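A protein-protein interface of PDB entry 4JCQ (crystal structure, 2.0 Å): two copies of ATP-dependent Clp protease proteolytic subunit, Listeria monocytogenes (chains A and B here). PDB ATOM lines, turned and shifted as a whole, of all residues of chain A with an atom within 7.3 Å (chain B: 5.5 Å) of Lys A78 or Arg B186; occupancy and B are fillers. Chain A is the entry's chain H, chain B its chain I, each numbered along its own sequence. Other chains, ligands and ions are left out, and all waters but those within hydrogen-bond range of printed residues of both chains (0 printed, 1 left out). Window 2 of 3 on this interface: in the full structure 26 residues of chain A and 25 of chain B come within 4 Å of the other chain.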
ATOM      1  N   LEU A  42      13.312  38.538  27.477  1.00  0.00           N
ATOM      2  CA  LEU A  42      13.201  37.078  27.453  1.00  0.00           C
ATOM      3  C   LEU A  42      13.873  36.420  28.658  1.00  0.00           C
ATOM      4  O   LEU A  42      13.335  35.466  29.226  1.00  0.00           O
ATOM      5  CB  LEU A  42      13.765  36.503  26.148  1.00  0.00           C
ATOM      6  CG  LEU A  42      13.008  36.776  24.842  1.00  0.00           C
ATOM      7  CD1 LEU A  42      13.774  36.206  23.656  1.00  0.00           C
ATOM      8  CD2 LEU A  42      11.589  36.220  24.877  1.00  0.00           C
ATOM      9  N   LEU A  43      15.040  36.934  29.042  1.00  0.00           N
ATOM     10  CA  LEU A  43      15.764  36.432  30.210  1.00  0.00           C
ATOM     11  C   LEU A  43      15.034  36.753  31.512  1.00  0.00           C
ATOM     12  O   LEU A  43      15.009  35.933  32.432  1.00  0.00           O
ATOM     13  CB  LEU A  43      17.195  36.981  30.245  1.00  0.00           C
ATOM     14  CG  LEU A  43      18.187  36.428  29.213  1.00  0.00           C
ATOM     15  CD1 LEU A  43      19.404  37.333  29.097  1.00  0.00           C
ATOM     16  CD2 LEU A  43      18.604  34.999  29.540  1.00  0.00           C
ATOM     17  N   GLU A  46      11.944  34.462  31.672  1.00  0.00           N
ATOM     18  CA  GLU A  46      12.424  33.117  31.987  1.00  0.00           C
ATOM     19  C   GLU A  46      12.708  32.950  33.481  1.00  0.00           C
ATOM     20  O   GLU A  46      12.365  31.924  34.070  1.00  0.00           O
ATOM     21  CB  GLU A  46      13.678  32.783  31.172  1.00  0.00           C
ATOM     22  CG  GLU A  46      14.272  31.416  31.485  1.00  0.00           C
ATOM     23  CD  GLU A  46      15.583  31.145  30.775  1.00  0.00           C
ATOM     24  OE1 GLU A  46      16.407  32.076  30.632  1.00  0.00           O
ATOM     25  OE2 GLU A  46      15.793  29.985  30.371  1.00  0.00           O
ATOM     26  N   SER A  47      13.327  33.965  34.085  1.00  0.00           N
ATOM     27  CA  SER A  47      13.682  33.927  35.505  1.00  0.00           C
ATOM     28  C   SER A  47      12.460  33.944  36.426  1.00  0.00           C
ATOM     29  O   SER A  47      12.525  33.460  37.557  1.00  0.00           O
ATOM     30  CB  SER A  47      14.628  35.077  35.859  1.00  0.00           C
ATOM     31  OG  SER A  47      13.959  36.326  35.825  1.00  0.00           O
ATOM     32  N   SER A  49       9.156  32.627  35.592  1.00  0.00           N
ATOM     33  CA  SER A  49       8.504  31.314  35.507  1.00  0.00           C
ATOM     34  C   SER A  49       8.801  30.591  34.194  1.00  0.00           C
ATOM     35  O   SER A  49       9.400  31.161  33.277  1.00  0.00           O
ATOM     36  CB  SER A  49       6.987  31.445  35.702  1.00  0.00           C
ATOM     37  OG  SER A  49       6.374  32.055  34.580  1.00  0.00           O
ATOM     38  N   ASN A  50       8.374  29.332  34.120  1.00  0.00           N
ATOM     39  CA  ASN A  50       8.484  28.528  32.905  1.00  0.00           C
ATOM     40  C   ASN A  50       7.242  28.619  32.016  1.00  0.00           C
ATOM     41  O   ASN A  50       7.134  27.905  31.018  1.00  0.00           O
ATOM     42  CB  ASN A  50       8.773  27.064  33.254  1.00  0.00           C
ATOM     43  CG  ASN A  50      10.196  26.844  33.736  1.00  0.00           C
ATOM     44  OD1 ASN A  50      10.417  26.220  34.773  1.00  0.00           O
ATOM     45  ND2 ASN A  50      11.167  27.351  32.984  1.00  0.00           N
ATOM     46  N   ASP A  51       6.311  29.500  32.386  1.00  0.00           N
ATOM     47  CA  ASP A  51       5.090  29.735  31.612  1.00  0.00           C
ATOM     48  C   ASP A  51       5.401  30.251  30.202  1.00  0.00           C
ATOM     49  O   ASP A  51       6.413  30.923  30.002  1.00  0.00           O
ATOM     50  CB  ASP A  51       4.176  30.723  32.346  1.00  0.00           C
ATOM     51  CG  ASP A  51       3.495  30.110  33.562  1.00  0.00           C
ATOM     52  OD1 ASP A  51       2.871  30.871  34.330  1.00  0.00           O
ATOM     53  OD2 ASP A  51       3.574  28.876  33.753  1.00  0.00           O
ATOM     54  N   ILE A  53       5.587  32.255  26.588  1.00  0.00           N
ATOM     55  CA  ILE A  53       5.767  33.661  26.229  1.00  0.00           C
ATOM     56  C   ILE A  53       5.199  33.891  24.830  1.00  0.00           C
ATOM     57  O   ILE A  53       5.397  33.070  23.932  1.00  0.00           O
ATOM     58  CB  ILE A  53       7.259  34.072  26.280  1.00  0.00           C
ATOM     59  CG1 ILE A  53       7.813  33.913  27.701  1.00  0.00           C
ATOM     60  CG2 ILE A  53       7.458  35.504  25.787  1.00  0.00           C
ATOM     61  CD1 ILE A  53       9.326  33.936  27.788  1.00  0.00           C
ATOM     62  N   MET A  73      18.093  33.130  21.026  1.00  0.00           N
ATOM     63  CA  MET A  73      17.624  33.391  22.393  1.00  0.00           C
ATOM     64  C   MET A  73      16.231  32.812  22.637  1.00  0.00           C
ATOM     65  O   MET A  73      15.945  32.313  23.729  1.00  0.00           O
ATOM     66  CB  MET A  73      17.645  34.890  22.720  1.00  0.00           C
ATOM     67  CG  MET A  73      19.032  35.467  22.988  1.00  0.00           C
ATOM     68  SD  MET A  73      19.958  34.692  24.336  1.00  0.00           S
ATOM     69  CE  MET A  73      18.810  34.837  25.699  1.00  0.00           C
ATOM     70  N   ILE A  74      15.378  32.883  21.614  1.00  0.00           N
ATOM     71  CA  ILE A  74      14.044  32.279  21.655  1.00  0.00           C
ATOM     72  C   ILE A  74      14.137  30.770  21.893  1.00  0.00           C
ATOM     73  O   ILE A  74      13.414  30.226  22.729  1.00  0.00           O
ATOM     74  CB  ILE A  74      13.236  32.594  20.370  1.00  0.00           C
ATOM     75  CG1 ILE A  74      12.744  34.047  20.392  1.00  0.00           C
ATOM     76  CG2 ILE A  74      12.053  31.645  20.210  1.00  0.00           C
ATOM     77  CD1 ILE A  74      12.293  34.573  19.043  1.00  0.00           C
ATOM     78  N   LYS A  75      15.038  30.107  21.170  1.00  0.00           N
ATOM     79  CA  LYS A  75      15.253  28.667  21.326  1.00  0.00           C
ATOM     80  C   LYS A  75      16.016  28.311  22.606  1.00  0.00           C
ATOM     81  O   LYS A  75      15.844  27.217  23.147  1.00  0.00           O
ATOM     82  CB  LYS A  75      15.975  28.089  20.105  1.00  0.00           C
ATOM     83  CG  LYS A  75      15.115  28.015  18.854  1.00  0.00           C
ATOM     84  CD  LYS A  75      15.718  27.073  17.825  1.00  0.00           C
ATOM     85  CE  LYS A  75      14.762  26.846  16.666  1.00  0.00           C
ATOM     86  NZ  LYS A  75      15.248  25.784  15.743  1.00  0.00           N
ATOM     87  N   PHE A  76      16.846  29.239  23.082  1.00  0.00           N
ATOM     88  CA  PHE A  76      17.702  29.013  24.252  1.00  0.00           C
ATOM     89  C   PHE A  76      16.927  28.938  25.568  1.00  0.00           C
ATOM     90  O   PHE A  76      17.165  28.042  26.381  1.00  0.00           O
ATOM     91  CB  PHE A  76      18.799  30.085  24.333  1.00  0.00           C
ATOM     92  CG  PHE A  76      19.710  29.944  25.521  1.00  0.00           C
ATOM     93  CD1 PHE A  76      20.714  28.978  25.537  1.00  0.00           C
ATOM     94  CD2 PHE A  76      19.573  30.785  26.623  1.00  0.00           C
ATOM     95  CE1 PHE A  76      21.556  28.849  26.633  1.00  0.00           C
ATOM     96  CE2 PHE A  76      20.413  30.659  27.721  1.00  0.00           C
ATOM     97  CZ  PHE A  76      21.406  29.691  27.724  1.00  0.00           C
ATOM     98  N   ILE A  77      16.011  29.881  25.772  1.00  0.00           N
ATOM     99  CA  ILE A  77      15.258  29.972  27.027  1.00  0.00           C
ATOM    100  C   ILE A  77      14.326  28.775  27.227  1.00  0.00           C
ATOM    101  O   ILE A  77      13.882  28.156  26.258  1.00  0.00           O
ATOM    102  CB  ILE A  77      14.478  31.306  27.151  1.00  0.00           C
ATOM    103  CG1 ILE A  77      13.476  31.471  25.999  1.00  0.00           C
ATOM    104  CG2 ILE A  77      15.449  32.482  27.225  1.00  0.00           C
ATOM    105  CD1 ILE A  77      12.480  32.596  26.191  1.00  0.00           C
ATOM    106  N   LYS A  78      14.050  28.449  28.488  1.00  0.00           N
ATOM    107  CA  LYS A  78      13.207  27.300  28.827  1.00  0.00           C
ATOM    108  C   LYS A  78      11.726  27.440  28.449  1.00  0.00           C
ATOM    109  O   LYS A  78      11.146  26.487  27.928  1.00  0.00           O
ATOM    110  CB  LYS A  78      13.367  26.907  30.303  1.00  0.00           C
ATOM    111  CG  LYS A  78      14.473  25.889  30.545  1.00  0.00           C
ATOM    112  CD  LYS A  78      14.603  25.509  32.014  1.00  0.00           C
ATOM    113  CE  LYS A  78      15.549  26.442  32.754  1.00  0.00           C
ATOM    114  NZ  LYS A  78      15.807  25.992  34.149  1.00  0.00           N
ATOM    115  N   PRO A  79      11.109  28.620  28.696  1.00  0.00           N
ATOM    116  CA  PRO A  79       9.693  28.769  28.335  1.00  0.00           C
ATOM    117  C   PRO A  79       9.412  28.551  26.846  1.00  0.00           C
ATOM    118  O   PRO A  79      10.238  28.897  25.997  1.00  0.00           O
ATOM    119  CB  PRO A  79       9.388  30.221  28.711  1.00  0.00           C
ATOM    120  CG  PRO A  79      10.370  30.549  29.778  1.00  0.00           C
ATOM    121  CD  PRO A  79      11.620  29.828  29.373  1.00  0.00           C
ATOM    122  N   THR A  80       8.252  27.968  26.551  1.00  0.00           N
ATOM    123  CA  THR A  80       7.783  27.806  25.178  1.00  0.00           C
ATOM    124  C   THR A  80       7.388  29.170  24.616  1.00  0.00           C
ATOM    125  O   THR A  80       6.667  29.931  25.262  1.00  0.00           O
ATOM    126  CB  THR A  80       6.585  26.836  25.107  1.00  0.00           C
ATOM    127  OG1 THR A  80       6.984  25.553  25.600  1.00  0.00           O
ATOM    128  CG2 THR A  80       6.082  26.681  23.676  1.00  0.00           C
ATOM    129  N   VAL A  81       7.873  29.472  23.415  1.00  0.00           N
ATOM    130  CA  VAL A  81       7.611  30.760  22.785  1.00  0.00           C
ATOM    131  C   VAL A  81       6.598  30.623  21.650  1.00  0.00           C
ATOM    132  O   VAL A  81       6.789  29.835  20.723  1.00  0.00           O
ATOM    133  CB  VAL A  81       8.913  31.422  22.277  1.00  0.00           C
ATOM    134  CG1 VAL A  81       8.609  32.673  21.463  1.00  0.00           C
ATOM    135  CG2 VAL A  81       9.832  31.761  23.446  1.00  0.00           C
ATOM    136  N   THR B  23      23.457  38.133  34.704  1.00  0.00           N
ATOM    137  CA  THR B  23      23.706  38.131  33.268  1.00  0.00           C
ATOM    138  C   THR B  23      24.101  39.531  32.801  1.00  0.00           C
ATOM    139  O   THR B  23      23.496  40.526  33.207  1.00  0.00           O
ATOM    140  CB  THR B  23      22.465  37.641  32.487  1.00  0.00           C
ATOM    141  OG1 THR B  23      22.113  36.322  32.924  1.00  0.00           O
ATOM    142  CG2 THR B  23      22.739  37.600  30.992  1.00  0.00           C
ATOM    143  N   PHE B  56      26.616  37.397  27.557  1.00  0.00           N
ATOM    144  CA  PHE B  56      26.266  37.186  26.152  1.00  0.00           C
ATOM    145  C   PHE B  56      26.933  38.271  25.314  1.00  0.00           C
ATOM    146  O   PHE B  56      26.742  39.463  25.569  1.00  0.00           O
ATOM    147  CB  PHE B  56      24.746  37.211  25.947  1.00  0.00           C
ATOM    148  CG  PHE B  56      24.024  36.033  26.550  1.00  0.00           C
ATOM    149  CD1 PHE B  56      23.619  36.051  27.881  1.00  0.00           C
ATOM    150  CD2 PHE B  56      23.735  34.909  25.780  1.00  0.00           C
ATOM    151  CE1 PHE B  56      22.951  34.968  28.436  1.00  0.00           C
ATOM    152  CE2 PHE B  56      23.065  33.824  26.329  1.00  0.00           C
ATOM    153  CZ  PHE B  56      22.673  33.853  27.660  1.00  0.00           C
ATOM    154  N   GLU B 184      22.352  24.973  22.312  1.00  0.00           N
ATOM    155  CA  GLU B 184      21.096  25.441  21.731  1.00  0.00           C
ATOM    156  C   GLU B 184      20.073  25.764  22.819  1.00  0.00           C
ATOM    157  O   GLU B 184      19.241  26.655  22.649  1.00  0.00           O
ATOM    158  CB  GLU B 184      20.532  24.392  20.766  1.00  0.00           C
ATOM    159  CG  GLU B 184      19.444  24.914  19.835  1.00  0.00           C
ATOM    160  CD  GLU B 184      18.785  23.818  19.015  1.00  0.00           C
ATOM    161  OE1 GLU B 184      17.558  23.903  18.794  1.00  0.00           O
ATOM    162  OE2 GLU B 184      19.485  22.873  18.590  1.00  0.00           O
ATOM    163  N   ASN B 185      20.150  25.038  23.933  1.00  0.00           N
ATOM    164  CA  ASN B 185      19.197  25.177  25.034  1.00  0.00           C
ATOM    165  C   ASN B 185      19.864  25.487  26.375  1.00  0.00           C
ATOM    166  O   ASN B 185      21.095  25.498  26.479  1.00  0.00           O
ATOM    167  CB  ASN B 185      18.340  23.911  25.154  1.00  0.00           C
ATOM    168  CG  ASN B 185      17.527  23.632  23.903  1.00  0.00           C
ATOM    169  OD1 ASN B 185      17.726  22.616  23.238  1.00  0.00           O
ATOM    170  ND2 ASN B 185      16.609  24.534  23.574  1.00  0.00           N
ATOM    171  N   ARG B 186      19.037  25.735  27.391  1.00  0.00           N
ATOM    172  CA  ARG B 186      19.497  26.069  28.743  1.00  0.00           C
ATOM    173  C   ARG B 186      20.309  24.973  29.426  1.00  0.00           C
ATOM    174  O   ARG B 186      21.287  25.265  30.119  1.00  0.00           O
ATOM    175  CB  ARG B 186      18.306  26.442  29.632  1.00  0.00           C
ATOM    176  CG  ARG B 186      18.046  27.932  29.740  1.00  0.00           C
ATOM    177  CD  ARG B 186      18.999  28.594  30.721  1.00  0.00           C
ATOM    178  NE  ARG B 186      18.784  30.038  30.791  1.00  0.00           N
ATOM    179  CZ  ARG B 186      19.650  30.906  31.305  1.00  0.00           C
ATOM    180  NH1 ARG B 186      20.810  30.492  31.801  1.00  0.00           N
ATOM    181  NH2 ARG B 186      19.357  32.197  31.318  1.00  0.00           N
ATOM    182  N   ASP B 187      19.897  23.720  29.230  1.00  0.00           N
ATOM    183  CA  ASP B 187      20.528  22.565  29.883  1.00  0.00           C
ATOM    184  C   ASP B 187      21.996  22.352  29.498  1.00  0.00           C
ATOM    185  O   ASP B 187      22.743  21.692  30.225  1.00  0.00           O
ATOM    186  CB  ASP B 187      19.709  21.288  29.643  1.00  0.00           C
ATOM    187  CG  ASP B 187      19.307  21.105  28.187  1.00  0.00           C
ATOM    188  OD1 ASP B 187      18.089  21.091  27.909  1.00  0.00           O
ATOM    189  OD2 ASP B 187      20.200  20.977  27.322  1.00  0.00           O
ATOM    190  N   GLY B 188      22.400  22.913  28.359  1.00  0.00           N
ATOM    191  CA  GLY B 188      23.790  22.858  27.906  1.00  0.00           C
ATOM    192  C   GLY B 188      24.712  23.795  28.669  1.00  0.00           C
ATOM    193  O   GLY B 188      25.933  23.620  28.656  1.00  0.00           O
ATOM    194  N   LEU B 189      24.124  24.789  29.333  1.00  0.00           N
ATOM    195  CA  LEU B 189      24.867  25.762  30.135  1.00  0.00           C
ATOM    196  C   LEU B 189      24.830  25.387  31.625  1.00  0.00           C
ATOM    197  O   LEU B 189      24.829  26.260  32.499  1.00  0.00           O
ATOM    198  CB  LEU B 189      24.295  27.171  29.904  1.00  0.00           C
ATOM    199  CG  LEU B 189      25.087  28.415  30.324  1.00  0.00           C
ATOM    200  CD1 LEU B 189      26.284  28.649  29.415  1.00  0.00           C
ATOM    201  CD2 LEU B 189      24.186  29.642  30.335  1.00  0.00           C
ATOM    202  N   LYS B 190      24.813  24.083  31.902  1.00  0.00           N
ATOM    203  CA  LYS B 190      24.691  23.566  33.269  1.00  0.00           C
ATOM    204  C   LYS B 190      25.904  23.892  34.149  1.00  0.00           C
ATOM    205  O   LYS B 190      27.011  24.127  33.661  1.00  0.00           O
ATOM    206  CB  LYS B 190      24.405  22.052  33.261  1.00  0.00           C
ATOM    207  CG  LYS B 190      25.614  21.128  33.111  1.00  0.00           C
ATOM    208  CD  LYS B 190      26.008  20.880  31.661  1.00  0.00           C
ATOM    209  CE  LYS B 190      27.191  21.739  31.244  1.00  0.00           C
ATOM    210  NZ  LYS B 190      27.609  21.474  29.840  1.00  0.00           N
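OE2 of Glu A46 is in salt-bridge range of NE of Arg B186, at 3.0 Å. The backbone carbonyl oxygen (O) of Lys A75 sits at hydrogen-bond distance from the side-chain amide nitrogen (ND2) of Asn B185 (2.8 Å). The backbone carbonyl oxygen (O) of Phe A76 is in hydrogen-bond range of the backbone NH (N) of Arg B186, 3.1 Å away. The backbone carbonyl oxygen (O) of Lys A75 lies close to the backbone carbonyl oxygen (O) of Glu B184 (3.5 Å).
The side-chain carboxylate of Glu A46 lies within hydrogen-bond range of the backbone NH of Lys A78 (3.0 Å).
Among the printed residues, pairs that only touch across the chains: Leu A43 with Thr B23 (3.8 Å), Leu A43 with Arg B186 (3.4 Å), Met A73 with Phe B56 (3.8 Å), Phe A76 with Phe B56 (3.9 Å), Phe A76 with Glu B184 (3.2 Å), Phe A76 with Asn B185 (3.4 Å), Phe A76 with Leu B189 (3.8 Å) and Lys A78 with Arg B186 (3.98 Å).
Printed residues of chain B within 4 Å of Leu A43: Thr B23 (3.8 Å) and Arg B186 (3.4 Å). Printed residues of chain B within 4 Å of Glu A46: Arg B186. Ile A77 touches none of the printed residues of chain B. Of the printed residues of chain A, Phe B56 touches Met A73 and Phe A76. Printed residues of chain A within 4 Å of Glu B184: Lys A75 and Phe A76. Arg B186 touches four residues of chain A. Printed residues of chain A within 4 Å of Leu B189: Phe A76 (3.8 Å). The nearest printed residue of chain B that does not touch Lys A78 is Asp B187 (6.0 Å). The nearest residue of chain A that does not touch Arg B186 is Ile A77 (4.4 Å). The nearest printed residue of chain A that does not touch Asn B185 is Ile A77 (5.3 Å).
Of the 9 printed residues of chain B, 6 touch a printed residue of chain A. Printed residues of chain A that touch a printed residue of chain B: Leu A43, Glu A46, Met A73, Lys A75, Phe A76 and Lys A78. Along chain A the printed residues that touch a printed residue of chain B span positions 43 to 78. Among the printed residues, 12 pairs touch across the chains.
No position is printed for both chains. Of the 12 pairs that touch across the chains among the printed residues, none has its exchanged pair printed and touching as well.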
